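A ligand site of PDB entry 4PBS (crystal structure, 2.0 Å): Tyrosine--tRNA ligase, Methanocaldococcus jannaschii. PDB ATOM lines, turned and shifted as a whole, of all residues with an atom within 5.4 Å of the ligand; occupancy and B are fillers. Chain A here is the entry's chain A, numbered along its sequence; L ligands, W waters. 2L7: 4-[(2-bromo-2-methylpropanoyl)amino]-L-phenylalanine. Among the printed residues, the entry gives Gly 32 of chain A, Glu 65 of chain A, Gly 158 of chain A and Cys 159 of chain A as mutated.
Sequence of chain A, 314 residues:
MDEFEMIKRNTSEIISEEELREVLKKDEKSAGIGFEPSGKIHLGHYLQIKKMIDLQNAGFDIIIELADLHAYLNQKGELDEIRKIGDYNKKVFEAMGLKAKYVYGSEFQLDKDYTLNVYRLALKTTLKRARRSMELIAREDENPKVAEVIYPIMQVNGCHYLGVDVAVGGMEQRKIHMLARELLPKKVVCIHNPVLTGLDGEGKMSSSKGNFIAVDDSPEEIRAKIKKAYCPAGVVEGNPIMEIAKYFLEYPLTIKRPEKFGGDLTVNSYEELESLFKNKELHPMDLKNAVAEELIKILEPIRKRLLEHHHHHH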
ATOM      1  N   GLY A  32      -3.300  17.832 -23.261  1.00  0.00           N
ATOM      2  CA  GLY A  32      -3.088  16.534 -22.666  1.00  0.00           C
ATOM      3  C   GLY A  32      -4.378  15.944 -22.123  1.00  0.00           C
ATOM      4  O   GLY A  32      -5.332  16.645 -21.820  1.00  0.00           O
ATOM      5  N   ILE A  33      -4.396  14.611 -22.051  1.00  0.00           N
ATOM      6  CA  ILE A  33      -5.507  13.873 -21.477  1.00  0.00           C
ATOM      7  C   ILE A  33      -4.937  12.535 -21.062  1.00  0.00           C
ATOM      8  O   ILE A  33      -4.000  12.041 -21.663  1.00  0.00           O
ATOM      9  CB  ILE A  33      -6.670  13.722 -22.494  1.00  0.00           C
ATOM     10  CG1 ILE A  33      -7.835  12.969 -21.852  1.00  0.00           C
ATOM     11  CG2 ILE A  33      -6.193  12.986 -23.734  1.00  0.00           C
ATOM     12  CD1 ILE A  33      -9.071  12.910 -22.708  1.00  0.00           C
ATOM     13  N   GLY A  34      -5.511  11.937 -20.029  1.00  0.00           N
ATOM     14  CA  GLY A  34      -5.081  10.640 -19.568  1.00  0.00           C
ATOM     15  C   GLY A  34      -6.234   9.659 -19.545  1.00  0.00           C
ATOM     16  O   GLY A  34      -7.393  10.050 -19.365  1.00  0.00           O
ATOM     17  N   PHE A  35      -5.903   8.379 -19.689  1.00  0.00           N
ATOM     18  CA  PHE A  35      -6.883   7.289 -19.653  1.00  0.00           C
ATOM     19  C   PHE A  35      -6.315   6.152 -18.819  1.00  0.00           C
ATOM     20  O   PHE A  35      -5.259   5.614 -19.163  1.00  0.00           O
ATOM     21  CB  PHE A  35      -7.197   6.747 -21.068  1.00  0.00           C
ATOM     22  CG  PHE A  35      -7.794   7.756 -22.005  1.00  0.00           C
ATOM     23  CD1 PHE A  35      -9.136   8.105 -21.914  1.00  0.00           C
ATOM     24  CD2 PHE A  35      -7.020   8.344 -23.009  1.00  0.00           C
ATOM     25  CE1 PHE A  35      -9.695   9.022 -22.792  1.00  0.00           C
ATOM     26  CE2 PHE A  35      -7.570   9.271 -23.886  1.00  0.00           C
ATOM     27  CZ  PHE A  35      -8.905   9.613 -23.780  1.00  0.00           C
ATOM     28  N   GLU A  36      -7.015   5.754 -17.777  1.00  0.00           N
ATOM     29  CA  GLU A  36      -6.702   4.474 -17.162  1.00  0.00           C
ATOM     30  C   GLU A  36      -6.956   3.407 -18.209  1.00  0.00           C
ATOM     31  O   GLU A  36      -8.045   3.391 -18.801  1.00  0.00           O
ATOM     32  CB  GLU A  36      -7.559   4.196 -15.926  1.00  0.00           C
ATOM     33  CG  GLU A  36      -7.406   5.184 -14.797  1.00  0.00           C
ATOM     34  CD  GLU A  36      -8.253   4.802 -13.597  1.00  0.00           C
ATOM     35  OE1 GLU A  36      -8.560   3.599 -13.428  1.00  0.00           O
ATOM     36  OE2 GLU A  36      -8.636   5.707 -12.830  1.00  0.00           O
ATOM     37  N   ILE A  63      -0.696  15.117 -26.156  1.00  0.00           N
ATOM     38  CA  ILE A  63      -0.026  14.198 -25.238  1.00  0.00           C
ATOM     39  C   ILE A  63      -1.114  13.325 -24.622  1.00  0.00           C
ATOM     40  O   ILE A  63      -2.051  13.847 -24.012  1.00  0.00           O
ATOM     41  CB  ILE A  63       0.750  14.940 -24.129  1.00  0.00           C
ATOM     42  CG1 ILE A  63       1.829  15.833 -24.751  1.00  0.00           C
ATOM     43  CG2 ILE A  63       1.385  13.941 -23.169  1.00  0.00           C
ATOM     44  CD1 ILE A  63       2.775  16.453 -23.751  1.00  0.00           C
ATOM     45  N   ILE A  64      -1.010  12.011 -24.807  1.00  0.00           N
ATOM     46  CA  ILE A  64      -1.959  11.067 -24.219  1.00  0.00           C
ATOM     47  C   ILE A  64      -1.234  10.301 -23.125  1.00  0.00           C
ATOM     48  O   ILE A  64      -0.232   9.618 -23.389  1.00  0.00           O
ATOM     49  CB  ILE A  64      -2.518  10.087 -25.265  1.00  0.00           C
ATOM     50  CG1 ILE A  64      -3.100  10.845 -26.468  1.00  0.00           C
ATOM     51  CG2 ILE A  64      -3.527   9.135 -24.624  1.00  0.00           C
ATOM     52  CD1 ILE A  64      -4.313  11.668 -26.159  1.00  0.00           C
ATOM     53  N   GLU A  65      -1.719  10.393 -21.889  1.00  0.00           N
ATOM     54  CA  GLU A  65      -1.137   9.609 -20.801  1.00  0.00           C
ATOM     55  C   GLU A  65      -1.848   8.264 -20.723  1.00  0.00           C
ATOM     56  O   GLU A  65      -3.058   8.211 -20.457  1.00  0.00           O
ATOM     57  CB  GLU A  65      -1.220  10.317 -19.454  1.00  0.00           C
ATOM     58  CG  GLU A  65      -0.565   9.450 -18.348  1.00  0.00           C
ATOM     59  CD  GLU A  65      -0.595  10.082 -16.962  1.00  0.00           C
ATOM     60  OE1 GLU A  65      -0.597   9.329 -15.960  1.00  0.00           O
ATOM     61  OE2 GLU A  65      -0.589  11.340 -16.877  1.00  0.00           O
ATOM     62  N   ALA A  67      -2.379   5.841 -18.403  1.00  0.00           N
ATOM     63  CA  ALA A  67      -2.238   6.116 -16.972  1.00  0.00           C
ATOM     64  C   ALA A  67      -2.212   4.808 -16.194  1.00  0.00           C
ATOM     65  O   ALA A  67      -3.125   4.471 -15.441  1.00  0.00           O
ATOM     66  CB  ALA A  67      -3.361   7.040 -16.504  1.00  0.00           C
ATOM     67  N   HIS A  70      -2.089   5.464 -12.302  1.00  0.00           N
ATOM     68  CA  HIS A  70      -3.405   5.841 -11.797  1.00  0.00           C
ATOM     69  C   HIS A  70      -4.342   4.637 -11.732  1.00  0.00           C
ATOM     70  O   HIS A  70      -5.075   4.466 -10.752  1.00  0.00           O
ATOM     71  CB  HIS A  70      -4.016   6.935 -12.671  1.00  0.00           C
ATOM     72  CG  HIS A  70      -3.489   8.309 -12.393  1.00  0.00           C
ATOM     73  ND1 HIS A  70      -3.973   9.086 -11.369  1.00  0.00           N
ATOM     74  CD2 HIS A  70      -2.553   9.054 -13.023  1.00  0.00           C
ATOM     75  CE1 HIS A  70      -3.339  10.248 -11.357  1.00  0.00           C
ATOM     76  NE2 HIS A  70      -2.478  10.250 -12.365  1.00  0.00           N
ATOM     77  N   PHE A 108       7.355   8.576 -15.703  1.00  0.00           N
ATOM     78  CA  PHE A 108       7.810   9.762 -14.980  1.00  0.00           C
ATOM     79  C   PHE A 108       7.242   9.907 -13.581  1.00  0.00           C
ATOM     80  O   PHE A 108       7.831  10.637 -12.772  1.00  0.00           O
ATOM     81  CB  PHE A 108       7.481  11.030 -15.788  1.00  0.00           C
ATOM     82  CG  PHE A 108       6.022  11.171 -16.157  1.00  0.00           C
ATOM     83  CD1 PHE A 108       5.521  10.571 -17.307  1.00  0.00           C
ATOM     84  CD2 PHE A 108       5.162  11.912 -15.357  1.00  0.00           C
ATOM     85  CE1 PHE A 108       4.194  10.690 -17.651  1.00  0.00           C
ATOM     86  CE2 PHE A 108       3.837  12.046 -15.686  1.00  0.00           C
ATOM     87  CZ  PHE A 108       3.339  11.435 -16.844  1.00  0.00           C
ATOM     88  N   GLN A 109       6.151   9.227 -13.250  1.00  0.00           N
ATOM     89  CA  GLN A 109       5.468   9.459 -11.991  1.00  0.00           C
ATOM     90  C   GLN A 109       6.161   8.830 -10.788  1.00  0.00           C
ATOM     91  O   GLN A 109       5.600   8.863  -9.680  1.00  0.00           O
ATOM     92  CB  GLN A 109       4.026   8.962 -12.107  1.00  0.00           C
ATOM     93  CG  GLN A 109       3.198   9.886 -12.932  1.00  0.00           C
ATOM     94  CD  GLN A 109       1.861   9.290 -13.329  1.00  0.00           C
ATOM     95  OE1 GLN A 109       1.663   8.073 -13.270  1.00  0.00           O
ATOM     96  NE2 GLN A 109       0.927  10.149 -13.723  1.00  0.00           N
ATOM     97  N   ILE A 137     -14.824   9.081  -9.799  1.00  0.00           N
ATOM     98  CA  ILE A 137     -13.683   8.410 -10.391  1.00  0.00           C
ATOM     99  C   ILE A 137     -13.311   7.145  -9.638  1.00  0.00           C
ATOM    100  O   ILE A 137     -12.862   6.159 -10.252  1.00  0.00           O
ATOM    101  CB  ILE A 137     -12.468   9.355 -10.470  1.00  0.00           C
ATOM    102  CG1 ILE A 137     -12.720  10.479 -11.448  1.00  0.00           C
ATOM    103  CG2 ILE A 137     -11.214   8.578 -10.831  1.00  0.00           C
ATOM    104  CD1 ILE A 137     -11.723  11.580 -11.291  1.00  0.00           C
ATOM    105  N   TYR A 151      -4.190   9.581  -5.679  1.00  0.00           N
ATOM    106  CA  TYR A 151      -4.576   9.670  -7.087  1.00  0.00           C
ATOM    107  C   TYR A 151      -4.745  11.109  -7.556  1.00  0.00           C
ATOM    108  O   TYR A 151      -4.084  11.536  -8.512  1.00  0.00           O
ATOM    109  CB  TYR A 151      -5.873   8.864  -7.291  1.00  0.00           C
ATOM    110  CG  TYR A 151      -6.375   8.690  -8.708  1.00  0.00           C
ATOM    111  CD1 TYR A 151      -6.900   9.752  -9.418  1.00  0.00           C
ATOM    112  CD2 TYR A 151      -6.384   7.445  -9.311  1.00  0.00           C
ATOM    113  CE1 TYR A 151      -7.416   9.588 -10.700  1.00  0.00           C
ATOM    114  CE2 TYR A 151      -6.879   7.259 -10.593  1.00  0.00           C
ATOM    115  CZ  TYR A 151      -7.391   8.335 -11.281  1.00  0.00           C
ATOM    116  OH  TYR A 151      -7.896   8.167 -12.541  1.00  0.00           O
ATOM    117  N   GLN A 155      -2.404  13.204 -10.315  1.00  0.00           N
ATOM    118  CA  GLN A 155      -2.902  13.749 -11.573  1.00  0.00           C
ATOM    119  C   GLN A 155      -2.618  15.243 -11.679  1.00  0.00           C
ATOM    120  O   GLN A 155      -2.239  15.727 -12.749  1.00  0.00           O
ATOM    121  CB  GLN A 155      -4.396  13.472 -11.711  1.00  0.00           C
ATOM    122  CG  GLN A 155      -5.002  13.808 -13.081  1.00  0.00           C
ATOM    123  CD  GLN A 155      -6.385  13.215 -13.280  1.00  0.00           C
ATOM    124  OE1 GLN A 155      -6.701  12.164 -12.724  1.00  0.00           O
ATOM    125  NE2 GLN A 155      -7.244  13.904 -14.038  1.00  0.00           N
ATOM    126  N   GLY A 158       0.929  15.592 -12.551  1.00  0.00           N
ATOM    127  CA  GLY A 158       1.131  15.238 -13.945  1.00  0.00           C
ATOM    128  C   GLY A 158       0.924  16.421 -14.867  1.00  0.00           C
ATOM    129  O   GLY A 158       1.709  16.644 -15.791  1.00  0.00           O
ATOM    130  N   CYS A 159      -0.141  17.196 -14.620  1.00  0.00           N
ATOM    131  CA  CYS A 159      -0.357  18.437 -15.361  1.00  0.00           C
ATOM    132  C   CYS A 159       0.869  19.331 -15.259  1.00  0.00           C
ATOM    133  O   CYS A 159       1.390  19.830 -16.266  1.00  0.00           O
ATOM    134  CB  CYS A 159      -1.575  19.189 -14.824  1.00  0.00           C
ATOM    135  SG  CYS A 159      -3.132  18.466 -15.274  1.00  0.00           S
ATOM    136  N   LEU A 162       4.049  17.554 -17.054  1.00  0.00           N
ATOM    137  CA  LEU A 162       3.975  17.522 -18.500  1.00  0.00           C
ATOM    138  C   LEU A 162       3.870  18.916 -19.112  1.00  0.00           C
ATOM    139  O   LEU A 162       4.095  19.042 -20.321  1.00  0.00           O
ATOM    140  CB  LEU A 162       2.803  16.666 -18.973  1.00  0.00           C
ATOM    141  CG  LEU A 162       2.997  15.184 -18.612  1.00  0.00           C
ATOM    142  CD1 LEU A 162       1.952  14.293 -19.246  1.00  0.00           C
ATOM    143  CD2 LEU A 162       4.395  14.744 -18.999  1.00  0.00           C
ATOM    144  N   VAL A 164       1.446  20.924 -19.973  1.00  0.00           N
ATOM    145  CA  VAL A 164       0.419  21.201 -20.974  1.00  0.00           C
ATOM    146  C   VAL A 164      -0.193  22.577 -20.742  1.00  0.00           C
ATOM    147  O   VAL A 164      -0.265  23.073 -19.616  1.00  0.00           O
ATOM    148  CB  VAL A 164      -0.667  20.117 -20.942  1.00  0.00           C
ATOM    149  CG1 VAL A 164      -0.100  18.759 -21.380  1.00  0.00           C
ATOM    150  CG2 VAL A 164      -1.268  19.998 -19.549  1.00  0.00           C
ATOM    151  N   ALA A 167      -5.789  20.956 -20.416  1.00  0.00           N
ATOM    152  CA  ALA A 167      -6.170  19.625 -19.969  1.00  0.00           C
ATOM    153  C   ALA A 167      -7.597  19.340 -20.431  1.00  0.00           C
ATOM    154  O   ALA A 167      -8.475  20.200 -20.347  1.00  0.00           O
ATOM    155  CB  ALA A 167      -6.058  19.493 -18.448  1.00  0.00           C
ATOM    156  N   VAL A 168      -7.804  18.146 -20.932  1.00  0.00           N
ATOM    157  CA  VAL A 168      -9.096  17.716 -21.442  1.00  0.00           C
ATOM    158  C   VAL A 168      -9.552  16.526 -20.625  1.00  0.00           C
ATOM    159  O   VAL A 168      -8.752  15.686 -20.214  1.00  0.00           O
ATOM    160  CB  VAL A 168      -9.012  17.359 -22.933  1.00  0.00           C
ATOM    161  CG1 VAL A 168     -10.389  16.927 -23.483  1.00  0.00           C
ATOM    162  CG2 VAL A 168      -8.440  18.524 -23.726  1.00  0.00           C
ATOM    163  N   GLU A 172     -16.322  14.492 -15.077  1.00  0.00           N
ATOM    164  CA  GLU A 172     -16.005  13.902 -13.788  1.00  0.00           C
ATOM    165  C   GLU A 172     -14.631  14.332 -13.288  1.00  0.00           C
ATOM    166  O   GLU A 172     -14.386  14.275 -12.076  1.00  0.00           O
ATOM    167  CB  GLU A 172     -16.080  12.370 -13.825  1.00  0.00           C
ATOM    168  CG  GLU A 172     -14.987  11.698 -14.624  1.00  0.00           C
ATOM    169  CD  GLU A 172     -15.235  11.732 -16.122  1.00  0.00           C
ATOM    170  OE1 GLU A 172     -14.307  11.335 -16.879  1.00  0.00           O
ATOM    171  OE2 GLU A 172     -16.362  12.118 -16.523  1.00  0.00           O
ATOM    172  N   GLN A 173     -13.756  14.792 -14.184  1.00  0.00           N
ATOM    173  CA  GLN A 173     -12.412  15.239 -13.847  1.00  0.00           C
ATOM    174  C   GLN A 173     -12.359  16.661 -13.337  1.00  0.00           C
ATOM    175  O   GLN A 173     -11.273  17.129 -12.974  1.00  0.00           O
ATOM    176  CB  GLN A 173     -11.476  15.123 -15.066  1.00  0.00           C
ATOM    177  CG  GLN A 173     -11.558  13.823 -15.868  1.00  0.00           C
ATOM    178  CD  GLN A 173     -11.181  12.633 -15.031  1.00  0.00           C
ATOM    179  OE1 GLN A 173     -10.176  12.643 -14.294  1.00  0.00           O
ATOM    180  NE2 GLN A 173     -11.998  11.586 -15.106  1.00  0.00           N
ATOM    181  N   ILE A 176     -10.779  17.457  -9.793  1.00  0.00           N
ATOM    182  CA  ILE A 176      -9.320  17.344  -9.848  1.00  0.00           C
ATOM    183  C   ILE A 176      -8.729  18.528 -10.624  1.00  0.00           C
ATOM    184  O   ILE A 176      -7.688  19.077 -10.243  1.00  0.00           O
ATOM    185  CB  ILE A 176      -8.883  16.015 -10.474  1.00  0.00           C
ATOM    186  CG1 ILE A 176      -9.191  14.872  -9.513  1.00  0.00           C
ATOM    187  CG2 ILE A 176      -7.369  16.067 -10.791  1.00  0.00           C
ATOM    188  CD1 ILE A 176      -8.918  13.488 -10.086  1.00  0.00           C
HETATM  189  N01 2L7 L   1      -8.558  10.414 -13.745  1.00  0.00           N
HETATM  190  C02 2L7 L   1      -8.624   9.822 -15.019  1.00  0.00           C
HETATM  191  C03 2L7 L   1      -7.384   9.338 -15.585  1.00  0.00           C
HETATM  192  C04 2L7 L   1      -6.251  10.250 -15.883  1.00  0.00           C
HETATM  193  C05 2L7 L   1      -6.553  11.528 -16.568  1.00  0.00           C
HETATM  194  C06 2L7 L   1      -5.454  12.448 -16.917  1.00  0.00           C
HETATM  195  C07 2L7 L   1      -4.060  12.125 -16.557  1.00  0.00           C
HETATM  196  N08 2L7 L   1      -3.005  12.987 -16.976  1.00  0.00           N
HETATM  197  C09 2L7 L   1      -3.172  14.150 -17.792  1.00  0.00           C
HETATM  198  C10 2L7 L   1      -1.957  14.863 -18.257  1.00  0.00           C
HETATM  199  C11 2L7 L   1      -2.229  16.313 -18.368  1.00  0.00           C
HETATM  200 BR1  2L7 L   1      -1.631  14.146 -20.035  1.00  0.00          BR
HETATM  201  C13 2L7 L   1      -0.777  14.533 -17.410  1.00  0.00           C
HETATM  202  O14 2L7 L   1      -4.258  14.604 -18.101  1.00  0.00           O
HETATM  203  C15 2L7 L   1      -3.727  10.821 -15.901  1.00  0.00           C
HETATM  204  C16 2L7 L   1      -4.842   9.885 -15.547  1.00  0.00           C
HETATM  205  C17 2L7 L   1      -9.681   8.845 -15.148  1.00  0.00           C
HETATM  206  O18 2L7 L   1      -9.564   7.897 -15.965  1.00  0.00           O
HETATM  207  O19 2L7 L   1     -10.682   8.951 -14.408  1.00  0.00           O
HETATM  208  O   HOH W   1     -10.187   6.972 -18.172  1.00  0.00           O
HETATM  209  O   HOH W   2      -9.479  11.748 -18.368  1.00  0.00           O
HETATM  210  O   HOH W   3      -6.442  15.618 -16.505  1.00  0.00           O
HETATM  211  O   HOH W   4      -7.921  14.167 -18.262  1.00  0.00           O
HETATM  212  O   HOH W   5     -12.320   6.485 -14.293  1.00  0.00           O
HETATM  213  O   HOH W   6      -0.714  12.359 -14.430  1.00  0.00           O
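A nitrogen (N01) of the ligand is in hydrogen-bond range of the side-chain amide oxygen (OE1) of Gln 155 (2.7 Å).
A nitrogen (N08) of the ligand lies within hydrogen-bond range of the side-chain carboxylate (OE2) of Glu 65 (2.9 Å).
OH of Tyr 151 sits at hydrogen-bond distance from N01 of the ligand (2.6 Å).
A nitrogen (N01) of the ligand lies within hydrogen-bond range of the side-chain amide oxygen of Gln 173, 2.8 Å away.
Water W1 lies within hydrogen-bond range of O18 of the ligand (2.5 Å) and N of Glu 36 (3.4 Å).
Water W3 lies within hydrogen-bond range of O14 of the ligand and NE2 of Gln 155.
Water W6 lies within hydrogen-bond range of the side-chain carboxylate of Glu 65, the side-chain amide nitrogen of Gln 109, a ring nitrogen (NE2) of His 70 and a nitrogen (N08) of the ligand.
OE1 of Gln 173 lies within hydrogen-bond range of NE2 of Gln 155, at 3.2 Å.
The side-chain amide nitrogen (NE2) of Gln 109 sits at hydrogen-bond distance from the side-chain carboxylate (OE1) of Glu 65 (2.8 Å).
The backbone NH (N) of Ile 33 lies within hydrogen-bond range of the backbone carbonyl oxygen (O) of Ile 63, at 3.2 Å.
The backbone NH (N) of Glu 65 is in hydrogen-bond range of the backbone carbonyl oxygen (O) of Ile 33.
The backbone carbonyl oxygen of Glu 65 lies within hydrogen-bond range of the backbone NH of Phe 35 (3.0 Å).
OH of Tyr 151 lies within hydrogen-bond range of OE2 of Glu 36, 2.6 Å away.
The backbone NH of Ala 67 lies within hydrogen-bond range of the backbone carbonyl oxygen of Phe 35, 3.0 Å away.
The side-chain carboxylate of Glu 172 lies within hydrogen-bond range of the side-chain amide nitrogen of Gln 173 (2.9 Å).
Gly 32 touches the ligand.
Ile 33 touches the ligand.
Gly 34 touches the ligand (N to C06, 3.2 Å).
CG of Glu 36 touches O18 of the ligand, at 3.7 Å.
Ala 67 touches the ligand (CB to C16, 3.3 Å).
His 70 touches the ligand.
Ile 137 touches the ligand (CG2 to O19, 3.6 Å).
Gly 158 touches the ligand (C to C13, 3.6 Å).
Cys 159 touches the ligand.
CD1 of Leu 162 touches C13 of the ligand, 3.3 Å away.
Val 164 touches the ligand (CG2 to C11, 3.99 Å).
Of the 24 residues printed, 15 come within 4 Å of the ligand.
Along chain A the residues within 4 Å of the ligand span positions 32 to 173.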
